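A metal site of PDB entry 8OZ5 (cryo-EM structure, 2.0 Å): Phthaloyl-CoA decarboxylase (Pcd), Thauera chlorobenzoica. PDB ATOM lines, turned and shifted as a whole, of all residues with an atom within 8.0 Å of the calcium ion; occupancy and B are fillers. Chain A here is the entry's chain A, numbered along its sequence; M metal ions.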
ATOM      1  N   ILE A  68      10.806 -16.525  33.683  1.00  0.00           N
ATOM      2  CA  ILE A  68      10.158 -15.287  33.264  1.00  0.00           C
ATOM      3  C   ILE A  68       9.473 -14.617  34.446  1.00  0.00           C
ATOM      4  O   ILE A  68       9.285 -13.386  34.451  1.00  0.00           O
ATOM      5  CB  ILE A  68       9.166 -15.563  32.131  1.00  0.00           C
ATOM      6  CG1 ILE A  68       8.798 -14.257  31.412  1.00  0.00           C
ATOM      7  CG2 ILE A  68       7.921 -16.252  32.649  1.00  0.00           C
ATOM      8  CD1 ILE A  68       9.967 -13.596  30.722  1.00  0.00           C
ATOM      9  N   SER A  80       2.534 -11.978  32.356  1.00  0.00           N
ATOM     10  CA  SER A  80       3.057 -11.901  30.994  1.00  0.00           C
ATOM     11  C   SER A  80       2.256 -10.934  30.143  1.00  0.00           C
ATOM     12  O   SER A  80       2.810 -10.241  29.289  1.00  0.00           O
ATOM     13  CB  SER A  80       3.083 -13.290  30.363  1.00  0.00           C
ATOM     14  OG  SER A  80       4.048 -14.119  30.986  1.00  0.00           O
ATOM     15  N   ARG A  83       3.283  -7.516  31.069  1.00  0.00           N
ATOM     16  CA  ARG A  83       4.603  -7.286  30.510  1.00  0.00           C
ATOM     17  C   ARG A  83       4.516  -6.940  29.025  1.00  0.00           C
ATOM     18  O   ARG A  83       5.173  -6.007  28.554  1.00  0.00           O
ATOM     19  CB  ARG A  83       5.489  -8.510  30.716  1.00  0.00           C
ATOM     20  CG  ARG A  83       6.696  -8.548  29.803  1.00  0.00           C
ATOM     21  CD  ARG A  83       7.589  -9.742  30.109  1.00  0.00           C
ATOM     22  NE  ARG A  83       6.913 -11.004  29.866  1.00  0.00           N
ATOM     23  CZ  ARG A  83       6.693 -11.512  28.654  1.00  0.00           C
ATOM     24  NH1 ARG A  83       7.096 -10.846  27.572  1.00  0.00           N
ATOM     25  NH2 ARG A  83       6.072 -12.676  28.519  1.00  0.00           N
ATOM     26  N   ALA A 322      15.754 -21.829  28.192  1.00  0.00           N
ATOM     27  CA  ALA A 322      14.669 -20.905  28.482  1.00  0.00           C
ATOM     28  C   ALA A 322      15.169 -19.476  28.628  1.00  0.00           C
ATOM     29  O   ALA A 322      14.426 -18.527  28.374  1.00  0.00           O
ATOM     30  CB  ALA A 322      13.929 -21.339  29.756  1.00  0.00           C
ATOM     31  N   ASP A 324      17.684 -17.848  26.782  1.00  0.00           N
ATOM     32  CA  ASP A 324      17.731 -17.263  25.448  1.00  0.00           C
ATOM     33  C   ASP A 324      16.328 -17.090  24.866  1.00  0.00           C
ATOM     34  O   ASP A 324      16.031 -16.073  24.210  1.00  0.00           O
ATOM     35  CB  ASP A 324      18.591 -18.135  24.532  1.00  0.00           C
ATOM     36  CG  ASP A 324      18.484 -17.761  23.075  1.00  0.00           C
ATOM     37  OD1 ASP A 324      19.319 -16.973  22.594  1.00  0.00           O
ATOM     38  OD2 ASP A 324      17.560 -18.259  22.392  1.00  0.00           O
ATOM     39  N   ALA A 325      15.469 -18.077  25.093  1.00  0.00           N
ATOM     40  CA  ALA A 325      14.110 -18.021  24.577  1.00  0.00           C
ATOM     41  C   ALA A 325      13.360 -16.817  25.129  1.00  0.00           C
ATOM     42  O   ALA A 325      12.703 -16.088  24.386  1.00  0.00           O
ATOM     43  CB  ALA A 325      13.369 -19.315  24.908  1.00  0.00           C
ATOM     44  N   ASN A 326      13.441 -16.602  26.452  1.00  0.00           N
ATOM     45  CA  ASN A 326      12.821 -15.422  27.043  1.00  0.00           C
ATOM     46  C   ASN A 326      13.419 -14.154  26.470  1.00  0.00           C
ATOM     47  O   ASN A 326      12.686 -13.250  26.025  1.00  0.00           O
ATOM     48  CB  ASN A 326      12.978 -15.463  28.561  1.00  0.00           C
ATOM     49  CG  ASN A 326      12.058 -16.456  29.219  1.00  0.00           C
ATOM     50  OD1 ASN A 326      10.933 -16.666  28.772  1.00  0.00           O
ATOM     51  ND2 ASN A 326      12.528 -17.087  30.290  1.00  0.00           N
ATOM     52  N   ILE A 327      14.758 -14.088  26.418  1.00  0.00           N
ATOM     53  CA  ILE A 327      15.488 -12.900  25.993  1.00  0.00           C
ATOM     54  C   ILE A 327      15.040 -12.443  24.618  1.00  0.00           C
ATOM     55  O   ILE A 327      14.882 -11.244  24.373  1.00  0.00           O
ATOM     56  CB  ILE A 327      17.002 -13.153  26.032  1.00  0.00           C
ATOM     57  CG1 ILE A 327      17.503 -13.163  27.469  1.00  0.00           C
ATOM     58  CG2 ILE A 327      17.729 -12.114  25.216  1.00  0.00           C
ATOM     59  CD1 ILE A 327      18.970 -13.490  27.595  1.00  0.00           C
ATOM     60  N   ASP A 328      14.838 -13.382  23.686  1.00  0.00           N
ATOM     61  CA  ASP A 328      14.358 -12.986  22.363  1.00  0.00           C
ATOM     62  C   ASP A 328      12.838 -12.796  22.311  1.00  0.00           C
ATOM     63  O   ASP A 328      12.336 -11.722  21.903  1.00  0.00           O
ATOM     64  CB  ASP A 328      14.770 -14.030  21.329  1.00  0.00           C
ATOM     65  CG  ASP A 328      16.279 -14.107  21.142  1.00  0.00           C
ATOM     66  OD1 ASP A 328      16.942 -13.065  21.289  1.00  0.00           O
ATOM     67  OD2 ASP A 328      16.788 -15.205  20.860  1.00  0.00           O
ATOM     68  N   THR A 329      12.089 -13.807  22.724  1.00  0.00           N
ATOM     69  CA  THR A 329      10.660 -13.829  22.480  1.00  0.00           C
ATOM     70  C   THR A 329       9.893 -12.786  23.282  1.00  0.00           C
ATOM     71  O   THR A 329       8.764 -12.478  22.914  1.00  0.00           O
ATOM     72  CB  THR A 329      10.091 -15.221  22.780  1.00  0.00           C
ATOM     73  OG1 THR A 329      10.188 -15.486  24.186  1.00  0.00           O
ATOM     74  CG2 THR A 329      10.856 -16.266  22.016  1.00  0.00           C
ATOM     75  N   SER A 330      10.470 -12.199  24.337  1.00  0.00           N
ATOM     76  CA  SER A 330       9.723 -11.199  25.083  1.00  0.00           C
ATOM     77  C   SER A 330       9.426  -9.965  24.237  1.00  0.00           C
ATOM     78  O   SER A 330       8.258  -9.607  24.021  1.00  0.00           O
ATOM     79  CB  SER A 330      10.501 -10.826  26.343  1.00  0.00           C
ATOM     80  OG  SER A 330      10.624 -11.948  27.201  1.00  0.00           O
ATOM     81  N   VAL A 331      10.465  -9.323  23.727  1.00  0.00           N
ATOM     82  CA  VAL A 331      10.221  -8.154  22.896  1.00  0.00           C
ATOM     83  C   VAL A 331       9.624  -8.574  21.554  1.00  0.00           C
ATOM     84  O   VAL A 331       8.904  -7.774  20.936  1.00  0.00           O
ATOM     85  CB  VAL A 331      11.498  -7.324  22.716  1.00  0.00           C
ATOM     86  CG1 VAL A 331      11.243  -6.151  21.782  1.00  0.00           C
ATOM     87  CG2 VAL A 331      11.978  -6.822  24.067  1.00  0.00           C
ATOM     88  N   ARG A 332       9.878  -9.801  21.095  1.00  0.00           N
ATOM     89  CA  ARG A 332       9.151 -10.263  19.909  1.00  0.00           C
ATOM     90  C   ARG A 332       7.636 -10.247  20.129  1.00  0.00           C
ATOM     91  O   ARG A 332       6.892  -9.766  19.270  1.00  0.00           O
ATOM     92  CB  ARG A 332       9.592 -11.666  19.511  1.00  0.00           C
ATOM     93  CG  ARG A 332      11.065 -11.798  19.258  1.00  0.00           C
ATOM     94  CD  ARG A 332      11.419 -11.329  17.860  1.00  0.00           C
ATOM     95  NE  ARG A 332      10.456 -11.758  16.851  1.00  0.00           N
ATOM     96  CZ  ARG A 332      10.221 -13.013  16.519  1.00  0.00           C
ATOM     97  NH1 ARG A 332      10.856 -14.006  17.123  1.00  0.00           N
ATOM     98  NH2 ARG A 332       9.324 -13.297  15.580  1.00  0.00           N
ATOM     99  N   GLU A 333       7.179 -10.778  21.266  1.00  0.00           N
ATOM    100  CA  GLU A 333       5.759 -10.772  21.589  1.00  0.00           C
ATOM    101  C   GLU A 333       5.226  -9.353  21.659  1.00  0.00           C
ATOM    102  O   GLU A 333       4.146  -9.050  21.139  1.00  0.00           O
ATOM    103  CB  GLU A 333       5.518 -11.489  22.922  1.00  0.00           C
ATOM    104  CG  GLU A 333       5.872 -12.952  22.933  1.00  0.00           C
ATOM    105  CD  GLU A 333       5.973 -13.509  24.343  1.00  0.00           C
ATOM    106  OE1 GLU A 333       5.910 -12.718  25.296  1.00  0.00           O
ATOM    107  OE2 GLU A 333       6.123 -14.737  24.489  1.00  0.00           O
ATOM    108  N   VAL A 351      -0.476 -12.029  23.057  1.00  0.00           N
ATOM    109  CA  VAL A 351       0.481 -12.651  22.158  1.00  0.00           C
ATOM    110  C   VAL A 351       1.495 -13.419  22.990  1.00  0.00           C
ATOM    111  O   VAL A 351       1.944 -12.938  24.036  1.00  0.00           O
ATOM    112  CB  VAL A 351       1.193 -11.602  21.272  1.00  0.00           C
ATOM    113  CG1 VAL A 351       2.226 -12.270  20.383  1.00  0.00           C
ATOM    114  CG2 VAL A 351       0.184 -10.849  20.433  1.00  0.00           C
ATOM    115  N   HIS A 352       1.841 -14.622  22.547  1.00  0.00           N
ATOM    116  CA  HIS A 352       2.744 -15.476  23.284  1.00  0.00           C
ATOM    117  C   HIS A 352       3.622 -16.245  22.310  1.00  0.00           C
ATOM    118  O   HIS A 352       3.119 -16.857  21.371  1.00  0.00           O
ATOM    119  CB  HIS A 352       1.977 -16.446  24.183  1.00  0.00           C
ATOM    120  CG  HIS A 352       2.858 -17.362  24.971  1.00  0.00           C
ATOM    121  ND1 HIS A 352       3.863 -16.916  25.782  1.00  0.00           N
ATOM    122  CD2 HIS A 352       2.878 -18.717  25.071  1.00  0.00           C
ATOM    123  CE1 HIS A 352       4.474 -17.938  26.349  1.00  0.00           C
ATOM    124  NE2 HIS A 352       3.893 -19.051  25.931  1.00  0.00           N
ATOM    125  N   ILE A 353       4.928 -16.204  22.550  1.00  0.00           N
ATOM    126  CA  ILE A 353       5.868 -17.028  21.803  1.00  0.00           C
ATOM    127  C   ILE A 353       6.429 -18.063  22.767  1.00  0.00           C
ATOM    128  O   ILE A 353       7.361 -17.764  23.524  1.00  0.00           O
ATOM    129  CB  ILE A 353       6.991 -16.187  21.167  1.00  0.00           C
ATOM    130  CG1 ILE A 353       6.400 -15.155  20.215  1.00  0.00           C
ATOM    131  CG2 ILE A 353       7.974 -17.082  20.443  1.00  0.00           C
ATOM    132  CD1 ILE A 353       7.420 -14.220  19.635  1.00  0.00           C
ATOM    133  N   PRO A 354       5.903 -19.282  22.779  1.00  0.00           N
ATOM    134  CA  PRO A 354       6.359 -20.274  23.744  1.00  0.00           C
ATOM    135  C   PRO A 354       7.784 -20.721  23.466  1.00  0.00           C
ATOM    136  O   PRO A 354       8.328 -20.543  22.384  1.00  0.00           O
ATOM    137  CB  PRO A 354       5.370 -21.437  23.554  1.00  0.00           C
ATOM    138  CG  PRO A 354       4.873 -21.271  22.177  1.00  0.00           C
ATOM    139  CD  PRO A 354       4.839 -19.800  21.907  1.00  0.00           C
ATOM    140  N   TYR A 355       8.394 -21.298  24.510  1.00  0.00           N
ATOM    141  CA  TYR A 355       9.750 -21.816  24.407  1.00  0.00           C
ATOM    142  C   TYR A 355       9.862 -22.833  23.271  1.00  0.00           C
ATOM    143  O   TYR A 355      10.865 -22.847  22.543  1.00  0.00           O
ATOM    144  CB  TYR A 355      10.148 -22.433  25.751  1.00  0.00           C
ATOM    145  CG  TYR A 355      11.558 -22.978  25.865  1.00  0.00           C
ATOM    146  CD1 TYR A 355      12.579 -22.567  25.022  1.00  0.00           C
ATOM    147  CD2 TYR A 355      11.863 -23.913  26.850  1.00  0.00           C
ATOM    148  CE1 TYR A 355      13.851 -23.076  25.140  1.00  0.00           C
ATOM    149  CE2 TYR A 355      13.137 -24.417  26.976  1.00  0.00           C
ATOM    150  CZ  TYR A 355      14.128 -23.995  26.127  1.00  0.00           C
ATOM    151  OH  TYR A 355      15.392 -24.507  26.260  1.00  0.00           O
ATOM    152  N   CYS A 356       8.848 -23.653  23.081  1.00  0.00           N
ATOM    153  CA  CYS A 356       8.876 -24.717  22.078  1.00  0.00           C
ATOM    154  C   CYS A 356       8.816 -24.196  20.649  1.00  0.00           C
ATOM    155  O   CYS A 356       8.870 -25.008  19.721  1.00  0.00           O
ATOM    156  CB  CYS A 356       7.719 -25.688  22.313  1.00  0.00           C
ATOM    157  SG  CYS A 356       6.087 -24.955  22.154  1.00  0.00           S
ATOM    158  N   ASP A 359      12.727 -19.278  18.750  1.00  0.00           N
ATOM    159  CA  ASP A 359      12.405 -17.872  18.980  1.00  0.00           C
ATOM    160  C   ASP A 359      11.885 -17.145  17.738  1.00  0.00           C
ATOM    161  O   ASP A 359      10.861 -16.446  17.805  1.00  0.00           O
ATOM    162  CB  ASP A 359      13.670 -17.168  19.461  1.00  0.00           C
ATOM    163  CG  ASP A 359      14.323 -17.901  20.603  1.00  0.00           C
ATOM    164  OD1 ASP A 359      14.933 -17.239  21.460  1.00  0.00           O
ATOM    165  OD2 ASP A 359      14.235 -19.154  20.642  1.00  0.00           O
ATOM    166  N   TYR A 405      -0.944 -20.069  27.126  1.00  0.00           N
ATOM    167  CA  TYR A 405       0.327 -20.527  27.661  1.00  0.00           C
ATOM    168  C   TYR A 405       0.438 -22.041  27.753  1.00  0.00           C
ATOM    169  O   TYR A 405       1.499 -22.550  28.138  1.00  0.00           O
ATOM    170  CB  TYR A 405       0.566 -19.918  29.049  1.00  0.00           C
ATOM    171  CG  TYR A 405       0.444 -18.416  29.061  1.00  0.00           C
ATOM    172  CD1 TYR A 405       1.410 -17.622  28.463  1.00  0.00           C
ATOM    173  CD2 TYR A 405      -0.645 -17.797  29.655  1.00  0.00           C
ATOM    174  CE1 TYR A 405       1.305 -16.247  28.474  1.00  0.00           C
ATOM    175  CE2 TYR A 405      -0.760 -16.420  29.668  1.00  0.00           C
ATOM    176  CZ  TYR A 405       0.211 -15.658  29.074  1.00  0.00           C
ATOM    177  OH  TYR A 405       0.106 -14.283  29.085  1.00  0.00           O
HETATM  178 CA    CA M   1       8.211 -16.288  25.361  1.00  0.00          CA
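The backbone carbonyl oxygen of Ala 325 lies close to the side-chain hydroxyl of Thr 329, 2.6 Å away. The side-chain carboxylate (OE2) of Glu 333 sits close to a ring nitrogen (ND1) of His 352, 3.4 Å away. NH1 of Arg 83 lies within salt-bridge range of OE1 of Glu 333 (3.2 Å).
Within 4 Å of the calcium ion: Thr 329, Glu 333 and Ile 353.
The calcium ion is bound by the side-chain hydroxyl of Thr 329 (2.4 Å), the backbone carbonyl oxygen of Ile 353 (2.5 Å) and the side-chain carboxylate of Glu 333 (2.7 Å). The calcium ion has three donor atoms within binding distance.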
